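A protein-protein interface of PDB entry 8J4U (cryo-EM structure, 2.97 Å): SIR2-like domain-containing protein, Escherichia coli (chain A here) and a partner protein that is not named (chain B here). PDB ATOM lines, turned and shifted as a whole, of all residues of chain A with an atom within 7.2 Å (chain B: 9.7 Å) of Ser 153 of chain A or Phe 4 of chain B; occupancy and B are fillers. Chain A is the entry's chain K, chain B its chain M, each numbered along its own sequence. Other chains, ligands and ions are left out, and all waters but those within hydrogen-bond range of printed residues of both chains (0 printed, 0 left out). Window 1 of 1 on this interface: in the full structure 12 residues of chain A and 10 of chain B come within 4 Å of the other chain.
O of Ser 149 of chain A lies close to OG of Ser 153 of chain A (3.2 Å).
Among the printed residues, pairs that only touch across the chains: Ser 153 of chain A with Phe 4 of chain B, Leu 180 of chain A with Leu 3 of chain B, Leu 180 of chain A with Phe 4 of chain B, Ile 182 of chain A with Phe 4 of chain B, Tyr 219 of chain A with Phe 4 of chain B, Tyr 219 of chain A with Leu 6 of chain B and Phe 390 of chain A with Phe 4 of chain B.
Of chain B, only Phe 4 comes within 4 Å of Ser 153 of chain A. Phe 4 of chain B touches just these residues of chain A: Ser 153 (3.6 Å), Leu 180 (3.8 Å), Ile 182 (3.9 Å), Tyr 219 (3.7 Å) and Phe 390 (3.96 Å). No residue of chain B comes within 4 Å of Gly 181 of chain A. Printed residues of chain A within 4 Å of Leu 3 of chain B: Leu 180 (3.9 Å). Of the printed residues of chain B, Leu 180 of chain A touches Leu 3 and Phe 4. Printed residues of chain B within 4 Å of Ile 182 of chain A: Phe 4 (3.9 Å). Printed residues of chain B within 4 Å of Phe 390 of chain A: Phe 4 (3.96 Å). Of the printed residues of chain A, Leu 6 of chain B touches Tyr 219 (3.2 Å). Gly 57 of chain B touches none of the printed residues of chain A. The nearest residue of chain B that does not touch Ser 153 of chain A is Gly 57 of chain B (4.1 Å). The nearest residue of chain A that does not touch Phe 4 of chain B is Ser 149 of chain A (4.04 Å).
Printed residues of chain B that touch a printed residue of chain A: Leu 3, Phe 4 and Leu 6. Hydrophobic or aromatic side chains of chain B within 4 Å of the printed part of chain A: Phe 4 and Leu 6. Of the 18 printed residues of chain A, 5 touch a printed residue of chain B. Among the printed residues, 7 pairs touch across the chains.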
ATOM      1  N   LYS A 145      -2.259  16.570  11.690  1.00  0.00           N
ATOM      2  CA  LYS A 145      -1.721  15.834  10.553  1.00  0.00           C
ATOM      3  C   LYS A 145      -0.248  16.143  10.335  1.00  0.00           C
ATOM      4  O   LYS A 145       0.544  15.238  10.044  1.00  0.00           O
ATOM      5  CB  LYS A 145      -2.511  16.180   9.296  1.00  0.00           C
ATOM      6  CG  LYS A 145      -4.000  16.001   9.436  1.00  0.00           C
ATOM      7  CD  LYS A 145      -4.655  15.779   8.095  1.00  0.00           C
ATOM      8  CE  LYS A 145      -6.100  16.220   8.089  1.00  0.00           C
ATOM      9  NZ  LYS A 145      -6.477  16.811   6.780  1.00  0.00           N
ATOM     10  N   LEU A 147       1.933  17.011  12.567  1.00  0.00           N
ATOM     11  CA  LEU A 147       2.688  16.318  13.604  1.00  0.00           C
ATOM     12  C   LEU A 147       3.009  14.886  13.185  1.00  0.00           C
ATOM     13  O   LEU A 147       4.173  14.470  13.163  1.00  0.00           O
ATOM     14  CB  LEU A 147       1.891  16.339  14.908  1.00  0.00           C
ATOM     15  CG  LEU A 147       2.507  15.666  16.131  1.00  0.00           C
ATOM     16  CD1 LEU A 147       3.746  16.402  16.578  1.00  0.00           C
ATOM     17  CD2 LEU A 147       1.484  15.616  17.236  1.00  0.00           C
ATOM     18  N   ILE A 148       1.968  14.118  12.863  1.00  0.00           N
ATOM     19  CA  ILE A 148       2.133  12.717  12.480  1.00  0.00           C
ATOM     20  C   ILE A 148       3.068  12.596  11.283  1.00  0.00           C
ATOM     21  O   ILE A 148       4.002  11.781  11.269  1.00  0.00           O
ATOM     22  CB  ILE A 148       0.763  12.088  12.182  1.00  0.00           C
ATOM     23  CG1 ILE A 148       0.060  11.714  13.482  1.00  0.00           C
ATOM     24  CG2 ILE A 148       0.918  10.875  11.301  1.00  0.00           C
ATOM     25  CD1 ILE A 148      -1.419  11.590  13.340  1.00  0.00           C
ATOM     26  N   SER A 149       2.788  13.369  10.231  1.00  0.00           N
ATOM     27  CA  SER A 149       3.561  13.252   9.002  1.00  0.00           C
ATOM     28  C   SER A 149       5.035  13.554   9.237  1.00  0.00           C
ATOM     29  O   SER A 149       5.906  12.849   8.718  1.00  0.00           O
ATOM     30  CB  SER A 149       2.980  14.178   7.938  1.00  0.00           C
ATOM     31  OG  SER A 149       3.938  14.488   6.945  1.00  0.00           O
ATOM     32  N   LYS A 150       5.339  14.598  10.011  1.00  0.00           N
ATOM     33  CA  LYS A 150       6.734  14.924  10.283  1.00  0.00           C
ATOM     34  C   LYS A 150       7.392  13.865  11.155  1.00  0.00           C
ATOM     35  O   LYS A 150       8.578  13.564  10.983  1.00  0.00           O
ATOM     36  CB  LYS A 150       6.842  16.289  10.958  1.00  0.00           C
ATOM     37  CG  LYS A 150       6.283  17.443  10.157  1.00  0.00           C
ATOM     38  CD  LYS A 150       7.013  18.719  10.487  1.00  0.00           C
ATOM     39  CE  LYS A 150       6.172  19.934  10.178  1.00  0.00           C
ATOM     40  NZ  LYS A 150       6.906  21.191  10.461  1.00  0.00           N
ATOM     41  N   LEU A 151       6.647  13.293  12.101  1.00  0.00           N
ATOM     42  CA  LEU A 151       7.235  12.270  12.958  1.00  0.00           C
ATOM     43  C   LEU A 151       7.597  11.030  12.154  1.00  0.00           C
ATOM     44  O   LEU A 151       8.645  10.417  12.386  1.00  0.00           O
ATOM     45  CB  LEU A 151       6.275  11.913  14.090  1.00  0.00           C
ATOM     46  CG  LEU A 151       6.241  12.859  15.292  1.00  0.00           C
ATOM     47  CD1 LEU A 151       5.219  12.390  16.302  1.00  0.00           C
ATOM     48  CD2 LEU A 151       7.607  12.980  15.935  1.00  0.00           C
ATOM     49  N   ILE A 152       6.742  10.641  11.211  1.00  0.00           N
ATOM     50  CA  ILE A 152       7.022   9.456  10.401  1.00  0.00           C
ATOM     51  C   ILE A 152       8.099   9.750   9.363  1.00  0.00           C
ATOM     52  O   ILE A 152       9.144   9.091   9.325  1.00  0.00           O
ATOM     53  CB  ILE A 152       5.737   8.938   9.735  1.00  0.00           C
ATOM     54  CG1 ILE A 152       4.857   8.237  10.767  1.00  0.00           C
ATOM     55  CG2 ILE A 152       6.088   8.003   8.603  1.00  0.00           C
ATOM     56  CD1 ILE A 152       3.543   7.785  10.238  1.00  0.00           C
ATOM     57  N   SER A 153       7.857  10.736   8.501  1.00  0.00           N
ATOM     58  CA  SER A 153       8.644  10.945   7.291  1.00  0.00           C
ATOM     59  C   SER A 153      10.145  11.035   7.528  1.00  0.00           C
ATOM     60  O   SER A 153      10.921  10.960   6.570  1.00  0.00           O
ATOM     61  CB  SER A 153       8.163  12.208   6.580  1.00  0.00           C
ATOM     62  OG  SER A 153       6.994  11.943   5.824  1.00  0.00           O
ATOM     63  N   ASN A 154      10.579  11.197   8.775  1.00  0.00           N
ATOM     64  CA  ASN A 154      12.005  11.217   9.093  1.00  0.00           C
ATOM     65  C   ASN A 154      12.298  10.083  10.068  1.00  0.00           C
ATOM     66  O   ASN A 154      12.406  10.277  11.278  1.00  0.00           O
ATOM     67  CB  ASN A 154      12.423  12.587   9.655  1.00  0.00           C
ATOM     68  CG  ASN A 154      11.621  12.994  10.868  1.00  0.00           C
ATOM     69  OD1 ASN A 154      10.823  12.219  11.393  1.00  0.00           O
ATOM     70  ND2 ASN A 154      11.826  14.224  11.316  1.00  0.00           N
ATOM     71  N   ARG A 155      12.451   8.888   9.502  1.00  0.00           N
ATOM     72  CA  ARG A 155      13.040   7.730  10.151  1.00  0.00           C
ATOM     73  C   ARG A 155      13.761   6.946   9.067  1.00  0.00           C
ATOM     74  O   ARG A 155      13.441   7.063   7.882  1.00  0.00           O
ATOM     75  CB  ARG A 155      11.998   6.836  10.845  1.00  0.00           C
ATOM     76  CG  ARG A 155      11.044   7.533  11.792  1.00  0.00           C
ATOM     77  CD  ARG A 155      11.742   8.115  13.009  1.00  0.00           C
ATOM     78  NE  ARG A 155      12.024   7.113  14.030  1.00  0.00           N
ATOM     79  CZ  ARG A 155      13.022   7.195  14.905  1.00  0.00           C
ATOM     80  NH1 ARG A 155      13.837   8.240  14.902  1.00  0.00           N
ATOM     81  NH2 ARG A 155      13.199   6.232  15.794  1.00  0.00           N
ATOM     82  N   GLN A 156      14.735   6.150   9.469  1.00  0.00           N
ATOM     83  CA  GLN A 156      15.518   5.351   8.546  1.00  0.00           C
ATOM     84  C   GLN A 156      15.242   3.869   8.738  1.00  0.00           C
ATOM     85  O   GLN A 156      14.654   3.453   9.742  1.00  0.00           O
ATOM     86  CB  GLN A 156      17.011   5.630   8.736  1.00  0.00           C
ATOM     87  CG  GLN A 156      17.367   7.103   8.759  1.00  0.00           C
ATOM     88  CD  GLN A 156      18.863   7.338   8.768  1.00  0.00           C
ATOM     89  OE1 GLN A 156      19.556   6.967   9.715  1.00  0.00           O
ATOM     90  NE2 GLN A 156      19.370   7.952   7.707  1.00  0.00           N
ATOM     91  N   LEU A 180      -5.276  10.667   6.515  1.00  0.00           N
ATOM     92  CA  LEU A 180      -3.959  10.543   5.900  1.00  0.00           C
ATOM     93  C   LEU A 180      -3.721   9.170   5.285  1.00  0.00           C
ATOM     94  O   LEU A 180      -2.887   9.050   4.382  1.00  0.00           O
ATOM     95  CB  LEU A 180      -2.848  10.802   6.915  1.00  0.00           C
ATOM     96  CG  LEU A 180      -2.523  12.237   7.302  1.00  0.00           C
ATOM     97  CD1 LEU A 180      -1.592  12.205   8.482  1.00  0.00           C
ATOM     98  CD2 LEU A 180      -1.891  12.974   6.150  1.00  0.00           C
ATOM     99  N   GLY A 181      -4.421   8.141   5.752  1.00  0.00           N
ATOM    100  CA  GLY A 181      -4.145   6.788   5.322  1.00  0.00           C
ATOM    101  C   GLY A 181      -3.091   6.085   6.142  1.00  0.00           C
ATOM    102  O   GLY A 181      -2.354   5.252   5.604  1.00  0.00           O
ATOM    103  N   ILE A 182      -2.993   6.398   7.430  1.00  0.00           N
ATOM    104  CA  ILE A 182      -2.018   5.797   8.317  1.00  0.00           C
ATOM    105  C   ILE A 182      -2.738   4.822   9.238  1.00  0.00           C
ATOM    106  O   ILE A 182      -3.957   4.879   9.420  1.00  0.00           O
ATOM    107  CB  ILE A 182      -1.257   6.873   9.126  1.00  0.00           C
ATOM    108  CG1 ILE A 182      -0.493   7.810   8.189  1.00  0.00           C
ATOM    109  CG2 ILE A 182      -0.307   6.243  10.118  1.00  0.00           C
ATOM    110  CD1 ILE A 182       0.794   7.245   7.671  1.00  0.00           C
ATOM    111  N   HIS A 218       6.007   0.677   6.060  1.00  0.00           N
ATOM    112  CA  HIS A 218       6.364   1.345   7.305  1.00  0.00           C
ATOM    113  C   HIS A 218       5.556   2.622   7.490  1.00  0.00           C
ATOM    114  O   HIS A 218       6.124   3.690   7.741  1.00  0.00           O
ATOM    115  CB  HIS A 218       7.860   1.661   7.336  1.00  0.00           C
ATOM    116  CG  HIS A 218       8.733   0.477   7.067  1.00  0.00           C
ATOM    117  ND1 HIS A 218       9.714   0.478   6.098  1.00  0.00           N
ATOM    118  CD2 HIS A 218       8.777  -0.747   7.643  1.00  0.00           C
ATOM    119  CE1 HIS A 218      10.324  -0.693   6.089  1.00  0.00           C
ATOM    120  NE2 HIS A 218       9.774  -1.456   7.017  1.00  0.00           N
ATOM    121  N   TYR A 219       4.234   2.522   7.370  1.00  0.00           N
ATOM    122  CA  TYR A 219       3.315   3.620   7.659  1.00  0.00           C
ATOM    123  C   TYR A 219       2.416   3.155   8.797  1.00  0.00           C
ATOM    124  O   TYR A 219       1.309   2.663   8.572  1.00  0.00           O
ATOM    125  CB  TYR A 219       2.493   4.013   6.422  1.00  0.00           C
ATOM    126  CG  TYR A 219       3.305   4.435   5.216  1.00  0.00           C
ATOM    127  CD1 TYR A 219       2.728   4.484   3.953  1.00  0.00           C
ATOM    128  CD2 TYR A 219       4.641   4.791   5.338  1.00  0.00           C
ATOM    129  CE1 TYR A 219       3.461   4.868   2.849  1.00  0.00           C
ATOM    130  CE2 TYR A 219       5.381   5.175   4.238  1.00  0.00           C
ATOM    131  CZ  TYR A 219       4.786   5.213   2.996  1.00  0.00           C
ATOM    132  OH  TYR A 219       5.516   5.596   1.896  1.00  0.00           O
ATOM    133  N   PRO A 387      10.831  17.592   5.835  1.00  0.00           N
ATOM    134  CA  PRO A 387      11.752  16.881   4.940  1.00  0.00           C
ATOM    135  C   PRO A 387      11.906  17.581   3.596  1.00  0.00           C
ATOM    136  O   PRO A 387      11.261  18.586   3.295  1.00  0.00           O
ATOM    137  CB  PRO A 387      11.107  15.501   4.775  1.00  0.00           C
ATOM    138  CG  PRO A 387      10.060  15.418   5.821  1.00  0.00           C
ATOM    139  CD  PRO A 387       9.607  16.812   6.067  1.00  0.00           C
ATOM    140  N   PHE A 390       9.428  15.252   0.568  1.00  0.00           N
ATOM    141  CA  PHE A 390       8.010  15.440   0.841  1.00  0.00           C
ATOM    142  C   PHE A 390       7.490  16.601  -0.002  1.00  0.00           C
ATOM    143  O   PHE A 390       8.048  17.703   0.059  1.00  0.00           O
ATOM    144  CB  PHE A 390       7.776  15.706   2.328  1.00  0.00           C
ATOM    145  CG  PHE A 390       6.349  15.521   2.761  1.00  0.00           C
ATOM    146  CD1 PHE A 390       5.393  16.465   2.440  1.00  0.00           C
ATOM    147  CD2 PHE A 390       5.968  14.415   3.505  1.00  0.00           C
ATOM    148  CE1 PHE A 390       4.082  16.309   2.836  1.00  0.00           C
ATOM    149  CE2 PHE A 390       4.655  14.255   3.906  1.00  0.00           C
ATOM    150  CZ  PHE A 390       3.712  15.206   3.570  1.00  0.00           C
ATOM    151  N   LEU B   3      -2.261   5.269   1.467  1.00  0.00           N
ATOM    152  CA  LEU B   3      -2.525   6.474   0.692  1.00  0.00           C
ATOM    153  C   LEU B   3      -1.496   7.557   1.002  1.00  0.00           C
ATOM    154  O   LEU B   3      -1.507   8.631   0.402  1.00  0.00           O
ATOM    155  CB  LEU B   3      -3.940   6.992   0.970  1.00  0.00           C
ATOM    156  CG  LEU B   3      -4.314   8.352   0.376  1.00  0.00           C
ATOM    157  CD1 LEU B   3      -4.076   8.364  -1.126  1.00  0.00           C
ATOM    158  CD2 LEU B   3      -5.759   8.706   0.693  1.00  0.00           C
ATOM    159  N   PHE B   4      -0.597   7.263   1.939  1.00  0.00           N
ATOM    160  CA  PHE B   4       0.395   8.244   2.354  1.00  0.00           C
ATOM    161  C   PHE B   4       1.395   8.494   1.231  1.00  0.00           C
ATOM    162  O   PHE B   4       1.999   7.556   0.701  1.00  0.00           O
ATOM    163  CB  PHE B   4       1.115   7.768   3.613  1.00  0.00           C
ATOM    164  CG  PHE B   4       1.982   8.816   4.248  1.00  0.00           C
ATOM    165  CD1 PHE B   4       1.459  10.052   4.585  1.00  0.00           C
ATOM    166  CD2 PHE B   4       3.320   8.568   4.505  1.00  0.00           C
ATOM    167  CE1 PHE B   4       2.253  11.019   5.166  1.00  0.00           C
ATOM    168  CE2 PHE B   4       4.117   9.532   5.088  1.00  0.00           C
ATOM    169  CZ  PHE B   4       3.583  10.759   5.419  1.00  0.00           C
ATOM    170  N   LYS B   5       1.571   9.765   0.871  1.00  0.00           N
ATOM    171  CA  LYS B   5       2.475  10.158  -0.209  1.00  0.00           C
ATOM    172  C   LYS B   5       3.798  10.605   0.407  1.00  0.00           C
ATOM    173  O   LYS B   5       4.091  11.794   0.541  1.00  0.00           O
ATOM    174  CB  LYS B   5       1.848  11.255  -1.064  1.00  0.00           C
ATOM    175  CG  LYS B   5       0.597  10.820  -1.807  1.00  0.00           C
ATOM    176  CD  LYS B   5       0.865   9.591  -2.658  1.00  0.00           C
ATOM    177  CE  LYS B   5       0.112   8.380  -2.131  1.00  0.00           C
ATOM    178  NZ  LYS B   5       0.170   7.237  -3.081  1.00  0.00           N
ATOM    179  N   LEU B   6       4.610   9.619   0.791  1.00  0.00           N
ATOM    180  CA  LEU B   6       5.907   9.919   1.383  1.00  0.00           C
ATOM    181  C   LEU B   6       6.914  10.405   0.347  1.00  0.00           C
ATOM    182  O   LEU B   6       7.888  11.069   0.714  1.00  0.00           O
ATOM    183  CB  LEU B   6       6.447   8.688   2.113  1.00  0.00           C
ATOM    184  CG  LEU B   6       7.659   8.887   3.028  1.00  0.00           C
ATOM    185  CD1 LEU B   6       7.659   7.854   4.142  1.00  0.00           C
ATOM    186  CD2 LEU B   6       8.957   8.819   2.245  1.00  0.00           C
ATOM    187  N   THR B   7       6.699  10.101  -0.933  1.00  0.00           N
ATOM    188  CA  THR B   7       7.621  10.510  -1.982  1.00  0.00           C
ATOM    189  C   THR B   7       6.871  10.634  -3.301  1.00  0.00           C
ATOM    190  O   THR B   7       6.001   9.816  -3.609  1.00  0.00           O
ATOM    191  CB  THR B   7       8.777   9.517  -2.143  1.00  0.00           C
ATOM    192  OG1 THR B   7       8.287   8.179  -2.008  1.00  0.00           O
ATOM    193  CG2 THR B   7       9.866   9.776  -1.113  1.00  0.00           C
ATOM    194  N   GLU B   8       7.224  11.662  -4.070  1.00  0.00           N
ATOM    195  CA  GLU B   8       6.699  11.889  -5.416  1.00  0.00           C
ATOM    196  C   GLU B   8       7.688  11.409  -6.471  1.00  0.00           C
ATOM    197  O   GLU B   8       7.828  12.014  -7.536  1.00  0.00           O
ATOM    198  CB  GLU B   8       6.378  13.369  -5.605  1.00  0.00           C
ATOM    199  CG  GLU B   8       5.711  13.722  -6.926  1.00  0.00           C
ATOM    200  CD  GLU B   8       4.982  15.050  -6.873  1.00  0.00           C
ATOM    201  OE1 GLU B   8       5.652  16.101  -6.957  1.00  0.00           O
ATOM    202  OE2 GLU B   8       3.739  15.043  -6.752  1.00  0.00           O
ATOM    203  N   ASP B  55      18.075   9.358  -0.505  1.00  0.00           N
ATOM    204  CA  ASP B  55      17.230   9.980   0.504  1.00  0.00           C
ATOM    205  C   ASP B  55      17.611   9.427   1.872  1.00  0.00           C
ATOM    206  O   ASP B  55      17.540   8.215   2.101  1.00  0.00           O
ATOM    207  CB  ASP B  55      15.751   9.734   0.204  1.00  0.00           C
ATOM    208  CG  ASP B  55      15.351   8.282   0.372  1.00  0.00           C
ATOM    209  OD1 ASP B  55      15.059   7.873   1.515  1.00  0.00           O
ATOM    210  OD2 ASP B  55      15.322   7.552  -0.640  1.00  0.00           O
ATOM    211  N   ALA B  56      18.031  10.315   2.774  1.00  0.00           N
ATOM    212  CA  ALA B  56      18.497   9.939   4.108  1.00  0.00           C
ATOM    213  C   ALA B  56      17.763  10.808   5.122  1.00  0.00           C
ATOM    214  O   ALA B  56      18.251  11.864   5.528  1.00  0.00           O
ATOM    215  CB  ALA B  56      20.008  10.091   4.216  1.00  0.00           C
ATOM    216  N   GLY B  57      16.586  10.352   5.536  1.00  0.00           N
ATOM    217  CA  GLY B  57      15.800  11.076   6.512  1.00  0.00           C
ATOM    218  C   GLY B  57      15.328  12.426   6.019  1.00  0.00           C
ATOM    219  O   GLY B  57      14.445  12.512   5.162  1.00  0.00           O
ATOM    220  N   ASN B  58      15.918  13.490   6.560  1.00  0.00           N
ATOM    221  CA  ASN B  58      15.497  14.854   6.284  1.00  0.00           C
ATOM    222  C   ASN B  58      16.432  15.585   5.330  1.00  0.00           C
ATOM    223  O   ASN B  58      16.315  16.805   5.182  1.00  0.00           O
ATOM    224  CB  ASN B  58      15.389  15.639   7.591  1.00  0.00           C
ATOM    225  CG  ASN B  58      16.696  15.674   8.355  1.00  0.00           C
ATOM    226  OD1 ASN B  58      17.449  14.700   8.361  1.00  0.00           O
ATOM    227  ND2 ASN B  58      16.976  16.799   8.998  1.00  0.00           N
ATOM    228  N   ILE B  59      17.362  14.879   4.690  1.00  0.00           N
ATOM    229  CA  ILE B  59      18.313  15.477   3.766  1.00  0.00           C
ATOM    230  C   ILE B  59      18.439  14.583   2.539  1.00  0.00           C
ATOM    231  O   ILE B  59      17.753  13.567   2.405  1.00  0.00           O
ATOM    232  CB  ILE B  59      19.691  15.718   4.419  1.00  0.00           C
ATOM    233  CG1 ILE B  59      20.408  14.398   4.702  1.00  0.00           C
ATOM    234  CG2 ILE B  59      19.532  16.506   5.700  1.00  0.00           C
ATOM    235  CD1 ILE B  59      21.827  14.581   5.163  1.00  0.00           C
